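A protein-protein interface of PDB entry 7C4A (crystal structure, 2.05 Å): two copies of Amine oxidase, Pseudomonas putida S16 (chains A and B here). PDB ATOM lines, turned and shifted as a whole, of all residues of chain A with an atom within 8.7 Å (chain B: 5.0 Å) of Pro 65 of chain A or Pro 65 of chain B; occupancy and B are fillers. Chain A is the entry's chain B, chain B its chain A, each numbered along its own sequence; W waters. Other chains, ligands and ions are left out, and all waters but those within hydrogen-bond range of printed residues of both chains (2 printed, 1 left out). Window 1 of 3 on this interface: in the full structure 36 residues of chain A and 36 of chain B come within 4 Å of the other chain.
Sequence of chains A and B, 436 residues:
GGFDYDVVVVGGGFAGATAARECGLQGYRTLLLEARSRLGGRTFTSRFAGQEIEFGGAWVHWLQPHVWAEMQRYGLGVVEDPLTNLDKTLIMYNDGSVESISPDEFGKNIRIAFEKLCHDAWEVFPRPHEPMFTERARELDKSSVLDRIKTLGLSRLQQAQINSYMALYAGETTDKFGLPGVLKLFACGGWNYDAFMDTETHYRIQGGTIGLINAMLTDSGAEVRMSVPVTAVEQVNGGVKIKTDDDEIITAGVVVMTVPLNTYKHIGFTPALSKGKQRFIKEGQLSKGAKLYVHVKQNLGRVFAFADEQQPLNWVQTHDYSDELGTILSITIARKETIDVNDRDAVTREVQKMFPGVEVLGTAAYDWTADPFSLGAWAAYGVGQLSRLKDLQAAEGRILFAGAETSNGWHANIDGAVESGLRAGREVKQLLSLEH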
ATOM      1  N   HIS A  61      -0.590  33.478 -10.311  1.00  0.00           N
ATOM      2  CA  HIS A  61      -1.736  34.357 -10.284  1.00  0.00           C
ATOM      3  C   HIS A  61      -3.007  33.567 -10.279  1.00  0.00           C
ATOM      4  O   HIS A  61      -3.034  32.452 -10.778  1.00  0.00           O
ATOM      5  CB  HIS A  61      -1.725  35.298 -11.485  1.00  0.00           C
ATOM      6  CG  HIS A  61      -2.528  36.543 -11.289  1.00  0.00           C
ATOM      7  ND1 HIS A  61      -3.879  36.600 -11.573  1.00  0.00           N
ATOM      8  CD2 HIS A  61      -2.165  37.787 -10.888  1.00  0.00           C
ATOM      9  CE1 HIS A  61      -4.314  37.830 -11.343  1.00  0.00           C
ATOM     10  NE2 HIS A  61      -3.294  38.570 -10.926  1.00  0.00           N
ATOM     11  N   TRP A  62      -4.062  34.151  -9.703  1.00  0.00           N
ATOM     12  CA  TRP A  62      -5.360  33.481  -9.619  1.00  0.00           C
ATOM     13  C   TRP A  62      -6.085  33.357 -10.958  1.00  0.00           C
ATOM     14  O   TRP A  62      -6.979  32.541 -11.070  1.00  0.00           O
ATOM     15  CB  TRP A  62      -6.290  34.137  -8.586  1.00  0.00           C
ATOM     16  CG  TRP A  62      -6.418  35.634  -8.750  1.00  0.00           C
ATOM     17  CD1 TRP A  62      -7.304  36.332  -9.538  1.00  0.00           C
ATOM     18  CD2 TRP A  62      -5.576  36.609  -8.124  1.00  0.00           C
ATOM     19  NE1 TRP A  62      -7.070  37.697  -9.405  1.00  0.00           N
ATOM     20  CE2 TRP A  62      -6.014  37.877  -8.537  1.00  0.00           C
ATOM     21  CE3 TRP A  62      -4.495  36.521  -7.240  1.00  0.00           C
ATOM     22  CZ2 TRP A  62      -5.403  39.045  -8.090  1.00  0.00           C
ATOM     23  CZ3 TRP A  62      -3.887  37.658  -6.809  1.00  0.00           C
ATOM     24  CH2 TRP A  62      -4.344  38.915  -7.221  1.00  0.00           C
ATOM     25  N   LEU A  63      -5.675  34.119 -11.979  1.00  0.00           N
ATOM     26  CA  LEU A  63      -6.157  33.914 -13.325  1.00  0.00           C
ATOM     27  C   LEU A  63      -5.571  32.663 -13.998  1.00  0.00           C
ATOM     28  O   LEU A  63      -5.951  32.342 -15.119  1.00  0.00           O
ATOM     29  CB  LEU A  63      -5.910  35.152 -14.192  1.00  0.00           C
ATOM     30  CG  LEU A  63      -6.644  36.406 -13.726  1.00  0.00           C
ATOM     31  CD1 LEU A  63      -6.243  37.616 -14.545  1.00  0.00           C
ATOM     32  CD2 LEU A  63      -8.151  36.189 -13.784  1.00  0.00           C
ATOM     33  N   GLN A  64      -4.636  31.994 -13.312  1.00  0.00           N
ATOM     34  CA  GLN A  64      -3.982  30.774 -13.782  1.00  0.00           C
ATOM     35  C   GLN A  64      -4.656  29.650 -12.992  1.00  0.00           C
ATOM     36  O   GLN A  64      -4.343  29.405 -11.847  1.00  0.00           O
ATOM     37  CB  GLN A  64      -2.476  30.844 -13.552  1.00  0.00           C
ATOM     38  CG  GLN A  64      -1.806  31.949 -14.365  1.00  0.00           C
ATOM     39  CD  GLN A  64      -0.367  32.215 -13.948  1.00  0.00           C
ATOM     40  OE1 GLN A  64       0.062  31.831 -12.848  1.00  0.00           O
ATOM     41  NE2 GLN A  64       0.367  32.911 -14.792  1.00  0.00           N
ATOM     42  N   PRO A  65      -5.667  28.985 -13.575  1.00  0.00           N
ATOM     43  CA  PRO A  65      -6.605  28.199 -12.791  1.00  0.00           C
ATOM     44  C   PRO A  65      -6.082  26.914 -12.145  1.00  0.00           C
ATOM     45  O   PRO A  65      -6.531  26.558 -11.065  1.00  0.00           O
ATOM     46  CB  PRO A  65      -7.702  27.885 -13.809  1.00  0.00           C
ATOM     47  CG  PRO A  65      -7.026  27.930 -15.161  1.00  0.00           C
ATOM     48  CD  PRO A  65      -5.958  28.986 -15.026  1.00  0.00           C
ATOM     49  N   HIS A  66      -5.155  26.218 -12.801  1.00  0.00           N
ATOM     50  CA  HIS A  66      -4.710  24.937 -12.305  1.00  0.00           C
ATOM     51  C   HIS A  66      -3.832  25.116 -11.081  1.00  0.00           C
ATOM     52  O   HIS A  66      -4.066  24.472 -10.043  1.00  0.00           O
ATOM     53  CB  HIS A  66      -4.028  24.128 -13.402  1.00  0.00           C
ATOM     54  CG  HIS A  66      -4.767  24.162 -14.703  1.00  0.00           C
ATOM     55  ND1 HIS A  66      -4.518  25.110 -15.678  1.00  0.00           N
ATOM     56  CD2 HIS A  66      -5.785  23.401 -15.164  1.00  0.00           C
ATOM     57  CE1 HIS A  66      -5.356  24.921 -16.689  1.00  0.00           C
ATOM     58  NE2 HIS A  66      -6.129  23.888 -16.408  1.00  0.00           N
ATOM     59  N   VAL A  67      -2.861  26.026 -11.164  1.00  0.00           N
ATOM     60  CA  VAL A  67      -2.000  26.274 -10.024  1.00  0.00           C
ATOM     61  C   VAL A  67      -2.770  26.932  -8.907  1.00  0.00           C
ATOM     62  O   VAL A  67      -2.554  26.593  -7.736  1.00  0.00           O
ATOM     63  CB  VAL A  67      -0.677  27.022 -10.373  1.00  0.00           C
ATOM     64  CG1 VAL A  67      -0.943  28.447 -10.826  1.00  0.00           C
ATOM     65  CG2 VAL A  67       0.284  26.979  -9.163  1.00  0.00           C
ATOM     66  N   TRP A  68      -3.696  27.844  -9.231  1.00  0.00           N
ATOM     67  CA  TRP A  68      -4.486  28.480  -8.162  1.00  0.00           C
ATOM     68  C   TRP A  68      -5.320  27.477  -7.347  1.00  0.00           C
ATOM     69  O   TRP A  68      -5.411  27.559  -6.102  1.00  0.00           O
ATOM     70  CB  TRP A  68      -5.379  29.629  -8.713  1.00  0.00           C
ATOM     71  CG  TRP A  68      -5.935  30.453  -7.633  1.00  0.00           C
ATOM     72  CD1 TRP A  68      -7.198  30.440  -7.150  1.00  0.00           C
ATOM     73  CD2 TRP A  68      -5.208  31.399  -6.841  1.00  0.00           C
ATOM     74  NE1 TRP A  68      -7.321  31.361  -6.096  1.00  0.00           N
ATOM     75  CE2 TRP A  68      -6.111  31.960  -5.907  1.00  0.00           C
ATOM     76  CE3 TRP A  68      -3.891  31.871  -6.885  1.00  0.00           C
ATOM     77  CZ2 TRP A  68      -5.738  32.953  -4.991  1.00  0.00           C
ATOM     78  CZ3 TRP A  68      -3.510  32.871  -5.954  1.00  0.00           C
ATOM     79  CH2 TRP A  68      -4.437  33.399  -5.039  1.00  0.00           C
ATOM     80  N   ALA A  69      -5.946  26.523  -8.041  1.00  0.00           N
ATOM     81  CA  ALA A  69      -6.725  25.467  -7.368  1.00  0.00           C
ATOM     82  C   ALA A  69      -5.862  24.618  -6.467  1.00  0.00           C
ATOM     83  O   ALA A  69      -6.282  24.267  -5.354  1.00  0.00           O
ATOM     84  CB  ALA A  69      -7.474  24.589  -8.374  1.00  0.00           C
ATOM     85  N   GLU A  70      -4.643  24.296  -6.904  1.00  0.00           N
ATOM     86  CA  GLU A  70      -3.709  23.541  -6.049  1.00  0.00           C
ATOM     87  C   GLU A  70      -3.338  24.317  -4.788  1.00  0.00           C
ATOM     88  O   GLU A  70      -3.196  23.756  -3.709  1.00  0.00           O
ATOM     89  CB  GLU A  70      -2.431  23.172  -6.791  1.00  0.00           C
ATOM     90  CG  GLU A  70      -2.578  22.236  -8.003  1.00  0.00           C
ATOM     91  CD  GLU A  70      -3.299  20.942  -7.682  1.00  0.00           C
ATOM     92  OE1 GLU A  70      -3.282  20.522  -6.499  1.00  0.00           O
ATOM     93  OE2 GLU A  70      -3.896  20.333  -8.601  1.00  0.00           O
ATOM     94  N   MET A  71      -3.216  25.635  -4.919  1.00  0.00           N
ATOM     95  CA  MET A  71      -2.867  26.468  -3.786  1.00  0.00           C
ATOM     96  C   MET A  71      -4.014  26.496  -2.781  1.00  0.00           C
ATOM     97  O   MET A  71      -3.772  26.515  -1.572  1.00  0.00           O
ATOM     98  CB  MET A  71      -2.485  27.867  -4.284  1.00  0.00           C
ATOM     99  CG  MET A  71      -1.110  27.884  -4.895  1.00  0.00           C
ATOM    100  SD  MET A  71      -0.808  29.534  -5.878  1.00  0.00           S
ATOM    101  CE  MET A  71      -0.709  30.793  -4.341  1.00  0.00           C
ATOM    102  N   GLN A  72      -5.262  26.462  -3.282  1.00  0.00           N
ATOM    103  CA  GLN A  72      -6.407  26.335  -2.393  1.00  0.00           C
ATOM    104  C   GLN A  72      -6.362  24.978  -1.679  1.00  0.00           C
ATOM    105  O   GLN A  72      -6.534  24.915  -0.470  1.00  0.00           O
ATOM    106  CB  GLN A  72      -7.725  26.506  -3.154  1.00  0.00           C
ATOM    107  CG  GLN A  72      -8.958  26.448  -2.274  1.00  0.00           C
ATOM    108  CD  GLN A  72      -9.008  27.545  -1.215  1.00  0.00           C
ATOM    109  OE1 GLN A  72      -9.369  27.268  -0.097  1.00  0.00           O
ATOM    110  NE2 GLN A  72      -8.674  28.784  -1.576  1.00  0.00           N
ATOM    111  N   ARG A  73      -6.093  23.908  -2.438  1.00  0.00           N
ATOM    112  CA  ARG A  73      -6.047  22.541  -1.891  1.00  0.00           C
ATOM    113  C   ARG A  73      -5.054  22.432  -0.755  1.00  0.00           C
ATOM    114  O   ARG A  73      -5.356  21.810   0.239  1.00  0.00           O
ATOM    115  CB  ARG A  73      -5.686  21.520  -2.971  1.00  0.00           C
ATOM    116  CG  ARG A  73      -5.426  20.094  -2.486  1.00  0.00           C
ATOM    117  CD  ARG A  73      -5.209  19.116  -3.675  1.00  0.00           C
ATOM    118  NE  ARG A  73      -6.493  18.789  -4.285  1.00  0.00           N
ATOM    119  CZ  ARG A  73      -6.939  19.200  -5.475  1.00  0.00           C
ATOM    120  NH1 ARG A  73      -6.206  19.922  -6.285  1.00  0.00           N
ATOM    121  NH2 ARG A  73      -8.161  18.865  -5.884  1.00  0.00           N
ATOM    122  N   HIS A 129      -8.005  28.376 -24.120  1.00  0.00           N
ATOM    123  CA  HIS A 129      -7.662  27.001 -23.839  1.00  0.00           C
ATOM    124  C   HIS A 129      -7.894  26.013 -24.996  1.00  0.00           C
ATOM    125  O   HIS A 129      -7.578  24.830 -24.852  1.00  0.00           O
ATOM    126  CB  HIS A 129      -8.296  26.540 -22.533  1.00  0.00           C
ATOM    127  CG  HIS A 129      -7.822  27.325 -21.362  1.00  0.00           C
ATOM    128  ND1 HIS A 129      -6.727  26.960 -20.608  1.00  0.00           N
ATOM    129  CD2 HIS A 129      -8.233  28.513 -20.870  1.00  0.00           C
ATOM    130  CE1 HIS A 129      -6.526  27.859 -19.666  1.00  0.00           C
ATOM    131  NE2 HIS A 129      -7.398  28.833 -19.827  1.00  0.00           N
ATOM    132  N   CYS A 188      -5.544  34.437 -22.311  1.00  0.00           N
ATOM    133  CA  CYS A 188      -5.674  33.749 -21.019  1.00  0.00           C
ATOM    134  C   CYS A 188      -5.781  34.731 -19.838  1.00  0.00           C
ATOM    135  O   CYS A 188      -6.426  34.438 -18.847  1.00  0.00           O
ATOM    136  CB  CYS A 188      -4.503  32.771 -20.762  1.00  0.00           C
ATOM    137  SG  CYS A 188      -4.480  31.265 -21.795  1.00  0.00           S
ATOM    138  N   GLY A 189      -5.139  35.904 -19.947  1.00  0.00           N
ATOM    139  CA  GLY A 189      -5.189  36.914 -18.881  1.00  0.00           C
ATOM    140  C   GLY A 189      -6.354  37.882 -19.023  1.00  0.00           C
ATOM    141  O   GLY A 189      -6.180  39.098 -18.934  1.00  0.00           O
ATOM    142  N   GLY A 409      -3.031  26.018 -22.300  1.00  0.00           N
ATOM    143  CA  GLY A 409      -3.248  27.357 -21.778  1.00  0.00           C
ATOM    144  C   GLY A 409      -1.972  28.134 -21.529  1.00  0.00           C
ATOM    145  O   GLY A 409      -1.343  28.643 -22.456  1.00  0.00           O
ATOM    146  N   TRP A 410      -1.600  28.221 -20.247  1.00  0.00           N
ATOM    147  CA  TRP A 410      -0.452  28.991 -19.798  1.00  0.00           C
ATOM    148  C   TRP A 410       0.855  28.179 -19.989  1.00  0.00           C
ATOM    149  O   TRP A 410       1.491  27.731 -19.038  1.00  0.00           O
ATOM    150  CB  TRP A 410      -0.651  29.366 -18.356  1.00  0.00           C
ATOM    151  CG  TRP A 410      -1.760  30.306 -18.097  1.00  0.00           C
ATOM    152  CD1 TRP A 410      -3.052  29.980 -17.796  1.00  0.00           C
ATOM    153  CD2 TRP A 410      -1.682  31.726 -18.028  1.00  0.00           C
ATOM    154  NE1 TRP A 410      -3.789  31.114 -17.599  1.00  0.00           N
ATOM    155  CE2 TRP A 410      -2.971  32.199 -17.709  1.00  0.00           C
ATOM    156  CE3 TRP A 410      -0.656  32.645 -18.214  1.00  0.00           C
ATOM    157  CZ2 TRP A 410      -3.260  33.565 -17.576  1.00  0.00           C
ATOM    158  CZ3 TRP A 410      -0.948  34.021 -18.088  1.00  0.00           C
ATOM    159  CH2 TRP A 410      -2.230  34.454 -17.772  1.00  0.00           C
ATOM    160  N   ASP A 415       1.641  27.031 -14.299  1.00  0.00           N
ATOM    161  CA  ASP A 415       0.260  26.620 -14.494  1.00  0.00           C
ATOM    162  C   ASP A 415       0.068  25.620 -15.626  1.00  0.00           C
ATOM    163  O   ASP A 415      -0.665  24.654 -15.472  1.00  0.00           O
ATOM    164  CB  ASP A 415      -0.653  27.818 -14.746  1.00  0.00           C
ATOM    165  CG  ASP A 415      -2.135  27.385 -14.828  1.00  0.00           C
ATOM    166  OD1 ASP A 415      -2.751  27.251 -13.753  1.00  0.00           O
ATOM    167  OD2 ASP A 415      -2.650  27.165 -15.952  1.00  0.00           O
ATOM    168  N   GLY A 416       0.725  25.840 -16.757  1.00  0.00           N
ATOM    169  CA  GLY A 416       0.657  24.912 -17.887  1.00  0.00           C
ATOM    170  C   GLY A 416       1.216  23.526 -17.544  1.00  0.00           C
ATOM    171  O   GLY A 416       0.681  22.538 -17.933  1.00  0.00           O
ATOM    172  N   VAL A 418       1.190  22.196 -14.488  1.00  0.00           N
ATOM    173  CA  VAL A 418       0.154  21.605 -13.657  1.00  0.00           C
ATOM    174  C   VAL A 418      -0.989  21.053 -14.507  1.00  0.00           C
ATOM    175  O   VAL A 418      -1.418  19.922 -14.312  1.00  0.00           O
ATOM    176  CB  VAL A 418      -0.355  22.585 -12.568  1.00  0.00           C
ATOM    177  CG1 VAL A 418      -1.501  21.980 -11.784  1.00  0.00           C
ATOM    178  CG2 VAL A 418       0.778  22.953 -11.622  1.00  0.00           C
ATOM    179  N   GLU A 419      -1.470  21.864 -15.448  1.00  0.00           N
ATOM    180  CA  GLU A 419      -2.507  21.464 -16.405  1.00  0.00           C
ATOM    181  C   GLU A 419      -2.189  20.113 -17.099  1.00  0.00           C
ATOM    182  O   GLU A 419      -3.032  19.197 -17.131  1.00  0.00           O
ATOM    183  CB  GLU A 419      -2.691  22.547 -17.482  1.00  0.00           C
ATOM    184  CG  GLU A 419      -3.714  22.178 -18.529  1.00  0.00           C
ATOM    185  CD  GLU A 419      -3.515  22.895 -19.870  1.00  0.00           C
ATOM    186  OE1 GLU A 419      -3.247  24.138 -19.873  1.00  0.00           O
ATOM    187  OE2 GLU A 419      -3.643  22.189 -20.937  1.00  0.00           O
ATOM    188  N   LEU A 422      -2.514  17.096 -14.801  1.00  0.00           N
ATOM    189  CA  LEU A 422      -3.903  16.705 -14.574  1.00  0.00           C
ATOM    190  C   LEU A 422      -4.378  15.873 -15.753  1.00  0.00           C
ATOM    191  O   LEU A 422      -5.046  14.859 -15.580  1.00  0.00           O
ATOM    192  CB  LEU A 422      -4.809  17.900 -14.358  1.00  0.00           C
ATOM    193  CG  LEU A 422      -4.521  18.801 -13.167  1.00  0.00           C
ATOM    194  CD1 LEU A 422      -5.440  19.993 -13.170  1.00  0.00           C
ATOM    195  CD2 LEU A 422      -4.670  18.054 -11.867  1.00  0.00           C
ATOM    196  N   TRP B  62     -13.388  29.589 -17.829  1.00  0.00           N
ATOM    197  CA  TRP B  62     -12.004  29.278 -17.458  1.00  0.00           C
ATOM    198  C   TRP B  62     -11.362  30.303 -16.520  1.00  0.00           C
ATOM    199  O   TRP B  62     -10.376  29.995 -15.894  1.00  0.00           O
ATOM    200  CB  TRP B  62     -11.093  29.073 -18.678  1.00  0.00           C
ATOM    201  CG  TRP B  62     -11.219  30.171 -19.722  1.00  0.00           C
ATOM    202  CD1 TRP B  62     -10.506  31.326 -19.796  1.00  0.00           C
ATOM    203  CD2 TRP B  62     -12.132  30.191 -20.807  1.00  0.00           C
ATOM    204  NE1 TRP B  62     -10.932  32.081 -20.864  1.00  0.00           N
ATOM    205  CE2 TRP B  62     -11.924  31.397 -21.507  1.00  0.00           C
ATOM    206  CE3 TRP B  62     -13.117  29.299 -21.262  1.00  0.00           C
ATOM    207  CZ2 TRP B  62     -12.675  31.740 -22.645  1.00  0.00           C
ATOM    208  CZ3 TRP B  62     -13.855  29.636 -22.391  1.00  0.00           C
ATOM    209  CH2 TRP B  62     -13.635  30.830 -23.067  1.00  0.00           C
ATOM    210  N   LEU B  63     -11.950  31.506 -16.407  1.00  0.00           N
ATOM    211  CA  LEU B  63     -11.519  32.462 -15.408  1.00  0.00           C
ATOM    212  C   LEU B  63     -11.952  32.063 -13.994  1.00  0.00           C
ATOM    213  O   LEU B  63     -11.623  32.764 -13.046  1.00  0.00           O
ATOM    214  CB  LEU B  63     -12.014  33.866 -15.768  1.00  0.00           C
ATOM    215  CG  LEU B  63     -11.395  34.418 -17.065  1.00  0.00           C
ATOM    216  CD1 LEU B  63     -11.976  35.777 -17.403  1.00  0.00           C
ATOM    217  CD2 LEU B  63      -9.865  34.500 -17.008  1.00  0.00           C
ATOM    218  N   GLN B  64     -12.751  30.984 -13.875  1.00  0.00           N
ATOM    219  CA  GLN B  64     -13.249  30.469 -12.621  1.00  0.00           C
ATOM    220  C   GLN B  64     -12.370  29.257 -12.311  1.00  0.00           C
ATOM    221  O   GLN B  64     -12.537  28.180 -12.881  1.00  0.00           O
ATOM    222  CB  GLN B  64     -14.729  30.130 -12.722  1.00  0.00           C
ATOM    223  CG  GLN B  64     -15.604  31.364 -12.978  1.00  0.00           C
ATOM    224  CD  GLN B  64     -17.035  31.018 -13.347  1.00  0.00           C
ATOM    225  OE1 GLN B  64     -17.336  29.888 -13.774  1.00  0.00           O
ATOM    226  NE2 GLN B  64     -17.931  31.985 -13.187  1.00  0.00           N
ATOM    227  N   PRO B  65     -11.320  29.426 -11.485  1.00  0.00           N
ATOM    228  CA  PRO B  65     -10.213  28.471 -11.468  1.00  0.00           C
ATOM    229  C   PRO B  65     -10.480  27.089 -10.911  1.00  0.00           C
ATOM    230  O   PRO B  65      -9.886  26.111 -11.389  1.00  0.00           O
ATOM    231  CB  PRO B  65      -9.146  29.219 -10.629  1.00  0.00           C
ATOM    232  CG  PRO B  65      -9.937  30.148  -9.748  1.00  0.00           C
ATOM    233  CD  PRO B  65     -11.130  30.559 -10.560  1.00  0.00           C
ATOM    234  N   HIS B  66     -11.326  26.990  -9.889  1.00  0.00           N
ATOM    235  CA  HIS B  66     -11.531  25.715  -9.206  1.00  0.00           C
ATOM    236  C   HIS B  66     -12.350  24.793 -10.095  1.00  0.00           C
ATOM    237  O   HIS B  66     -11.982  23.641 -10.277  1.00  0.00           O
ATOM    238  CB  HIS B  66     -12.183  25.936  -7.840  1.00  0.00           C
ATOM    239  CG  HIS B  66     -11.544  27.051  -7.062  1.00  0.00           C
ATOM    240  ND1 HIS B  66     -11.997  28.354  -7.121  1.00  0.00           N
ATOM    241  CD2 HIS B  66     -10.444  27.066  -6.259  1.00  0.00           C
ATOM    242  CE1 HIS B  66     -11.197  29.125  -6.389  1.00  0.00           C
ATOM    243  NE2 HIS B  66     -10.261  28.364  -5.843  1.00  0.00           N
ATOM    244  N   VAL B  67     -13.445  25.308 -10.679  1.00  0.00           N
ATOM    245  CA  VAL B  67     -14.263  24.466 -11.543  1.00  0.00           C
ATOM    246  C   VAL B  67     -13.520  24.152 -12.825  1.00  0.00           C
ATOM    247  O   VAL B  67     -13.606  23.043 -13.334  1.00  0.00           O
ATOM    248  CB  VAL B  67     -15.689  25.031 -11.810  1.00  0.00           C
ATOM    249  CG1 VAL B  67     -15.651  26.331 -12.612  1.00  0.00           C
ATOM    250  CG2 VAL B  67     -16.562  23.964 -12.488  1.00  0.00           C
ATOM    251  N   TRP B  68     -12.757  25.111 -13.359  1.00  0.00           N
ATOM    252  CA  TRP B  68     -12.017  24.857 -14.589  1.00  0.00           C
ATOM    253  C   TRP B  68     -10.978  23.717 -14.413  1.00  0.00           C
ATOM    254  O   TRP B  68     -10.823  22.856 -15.300  1.00  0.00           O
ATOM    255  CB  TRP B  68     -11.343  26.131 -15.136  1.00  0.00           C
ATOM    256  CG  TRP B  68     -10.828  25.938 -16.491  1.00  0.00           C
ATOM    257  CD1 TRP B  68      -9.532  25.743 -16.872  1.00  0.00           C
ATOM    258  CD2 TRP B  68     -11.621  25.867 -17.676  1.00  0.00           C
ATOM    259  NE1 TRP B  68      -9.476  25.570 -18.264  1.00  0.00           N
ATOM    260  CE2 TRP B  68     -10.746  25.642 -18.766  1.00  0.00           C
ATOM    261  CE3 TRP B  68     -12.993  25.985 -17.916  1.00  0.00           C
ATOM    262  CZ2 TRP B  68     -11.191  25.530 -20.081  1.00  0.00           C
ATOM    263  CZ3 TRP B  68     -13.452  25.855 -19.249  1.00  0.00           C
ATOM    264  CH2 TRP B  68     -12.543  25.642 -20.304  1.00  0.00           C
ATOM    265  N   ALA B  69     -10.277  23.716 -13.275  1.00  0.00           N
ATOM    266  CA  ALA B  69      -9.306  22.668 -12.985  1.00  0.00           C
ATOM    267  C   ALA B  69      -9.967  21.297 -12.871  1.00  0.00           C
ATOM    268  O   ALA B  69      -9.417  20.306 -13.346  1.00  0.00           O
ATOM    269  CB  ALA B  69      -8.515  22.987 -11.711  1.00  0.00           C
ATOM    270  N   HIS B 129      -9.663  37.291  -4.262  1.00  0.00           N
ATOM    271  CA  HIS B 129      -9.785  36.130  -3.383  1.00  0.00           C
ATOM    272  C   HIS B 129      -9.456  36.398  -1.895  1.00  0.00           C
ATOM    273  O   HIS B 129      -9.598  35.515  -1.103  1.00  0.00           O
ATOM    274  CB  HIS B 129      -8.988  34.947  -3.936  1.00  0.00           C
ATOM    275  CG  HIS B 129      -9.467  34.525  -5.279  1.00  0.00           C
ATOM    276  ND1 HIS B 129     -10.398  33.522  -5.447  1.00  0.00           N
ATOM    277  CD2 HIS B 129      -9.230  35.028  -6.512  1.00  0.00           C
ATOM    278  CE1 HIS B 129     -10.667  33.398  -6.734  1.00  0.00           C
ATOM    279  NE2 HIS B 129     -10.000  34.320  -7.398  1.00  0.00           N
ATOM    280  N   TRP B 410     -15.650  33.270  -6.241  1.00  0.00           N
ATOM    281  CA  TRP B 410     -16.874  33.294  -7.053  1.00  0.00           C
ATOM    282  C   TRP B 410     -18.061  32.764  -6.248  1.00  0.00           C
ATOM    283  O   TRP B 410     -18.570  31.666  -6.486  1.00  0.00           O
ATOM    284  CB  TRP B 410     -16.656  32.529  -8.327  1.00  0.00           C
ATOM    285  CG  TRP B 410     -15.674  33.086  -9.262  1.00  0.00           C
ATOM    286  CD1 TRP B 410     -14.356  32.834  -9.305  1.00  0.00           C
ATOM    287  CD2 TRP B 410     -15.951  33.968 -10.357  1.00  0.00           C
ATOM    288  NE1 TRP B 410     -13.765  33.518 -10.353  1.00  0.00           N
ATOM    289  CE2 TRP B 410     -14.734  34.199 -11.030  1.00  0.00           C
ATOM    290  CE3 TRP B 410     -17.126  34.540 -10.862  1.00  0.00           C
ATOM    291  CZ2 TRP B 410     -14.636  35.019 -12.150  1.00  0.00           C
ATOM    292  CZ3 TRP B 410     -17.046  35.348 -11.984  1.00  0.00           C
ATOM    293  CH2 TRP B 410     -15.805  35.604 -12.606  1.00  0.00           C
ATOM    294  N   ASP B 415     -18.263  27.663  -9.084  1.00  0.00           N
ATOM    295  CA  ASP B 415     -16.862  27.730  -8.737  1.00  0.00           C
ATOM    296  C   ASP B 415     -16.616  27.953  -7.250  1.00  0.00           C
ATOM    297  O   ASP B 415     -15.754  27.306  -6.680  1.00  0.00           O
ATOM    298  CB  ASP B 415     -16.123  28.812  -9.521  1.00  0.00           C
ATOM    299  CG  ASP B 415     -14.630  28.815  -9.217  1.00  0.00           C
ATOM    300  OD1 ASP B 415     -13.916  28.023  -9.881  1.00  0.00           O
ATOM    301  OD2 ASP B 415     -14.184  29.602  -8.329  1.00  0.00           O
HETATM  302  O   HOH W   1      -8.869  29.941  -4.065  1.00  0.00           O
HETATM  303  O   HOH W   2      -7.657  23.259 -18.723  1.00  0.00           O
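Pro 65 of chain B touches its own counterpart, Pro 65 of chain A. Pro 65 of chain A touches Trp 68 of chain B, and with the chains exchanged Trp 68 of chain A touches Pro 65 of chain B. His 66 of chain A touches Trp 68 of chain B, and with the chains exchanged Trp 68 of chain A touches His 66 of chain B. Trp 68 of chain A touches His 129 of chain B, and with the chains exchanged His 129 of chain A touches Trp 68 of chain B. Of the 14 pairs that touch across the chains among the printed residues, 12 have their exchanged pair printed and touching as well.
Water W1 lies within hydrogen-bond range of NE2 of Gln 72 of chain A (2.8 Å), NE2 of His 66 of chain B (2.8 Å) and NE1 of Trp 68 of chain A (2.9 Å). Water W2 lies within hydrogen-bond range of a ring nitrogen (NE2) of His 66 of chain A and the indole nitrogen (NE1) of Trp 68 of chain B.
The backbone NH (N) of His 66 of chain A is in hydrogen-bond range of the side-chain carboxylate (OD1) of Asp 415 of chain A (2.8 Å). The backbone NH (N) of His 66 of chain B sits at hydrogen-bond distance from the side-chain carboxylate (OD1) of Asp 415 of chain B (2.8 Å).
The backbone carbonyl oxygen (O) of Pro 65 of chain A lies close to the backbone carbonyl oxygen (O) of Pro 65 of chain B (3.4 Å).
Trp 62 of chain A touches His 129 of chain B (CG to CD2, 3.6 Å). Pro 65 of chain A touches Trp 62 of chain B (CB to O, 3.99 Å). Pro 65 of chain A touches Trp 68 of chain B. NE2 of His 66 of chain A touches CD1 of Trp 68 of chain B (3.9 Å). Trp 68 of chain A touches Pro 65 of chain B. CD1 of Trp 68 of chain A touches NE2 of His 66 of chain B, 3.9 Å away. CB of Ala 69 of chain B touches CB of Ala 69 of chain A (3.8 Å). His 129 of chain A touches Trp 62 of chain B. CD1 of Leu 422 of chain A touches O of Ala 69 of chain B, at 3.99 Å.
Of the 23 printed residues of chain A, 8 touch a printed residue of chain B. Hydrophobic or aromatic side chains of chain A that line the printed part of chain B: Trp 62, Pro 65, His 66, Trp 68, Ala 69, His 129 and Leu 422. Along chain B the printed residues that touch a printed residue of chain A span positions 62 to 129. Among the printed residues, 14 pairs touch across the chains.
Of the printed residues of chain B, Trp 68 of chain A touches Pro 65 (3.8 Å), His 66 (3.9 Å) and His 129 (3.8 Å). Of the printed residues of chain A, Pro 65 of chain B touches Trp 62, Pro 65 and Trp 68. Printed residues of chain A within 4 Å of Trp 68 of chain B: Pro 65 (3.7 Å), His 66 (3.9 Å) and His 129 (3.9 Å). The nearest printed residue of chain B that does not touch Pro 65 of chain A is Ala 69 of chain B (4.1 Å).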
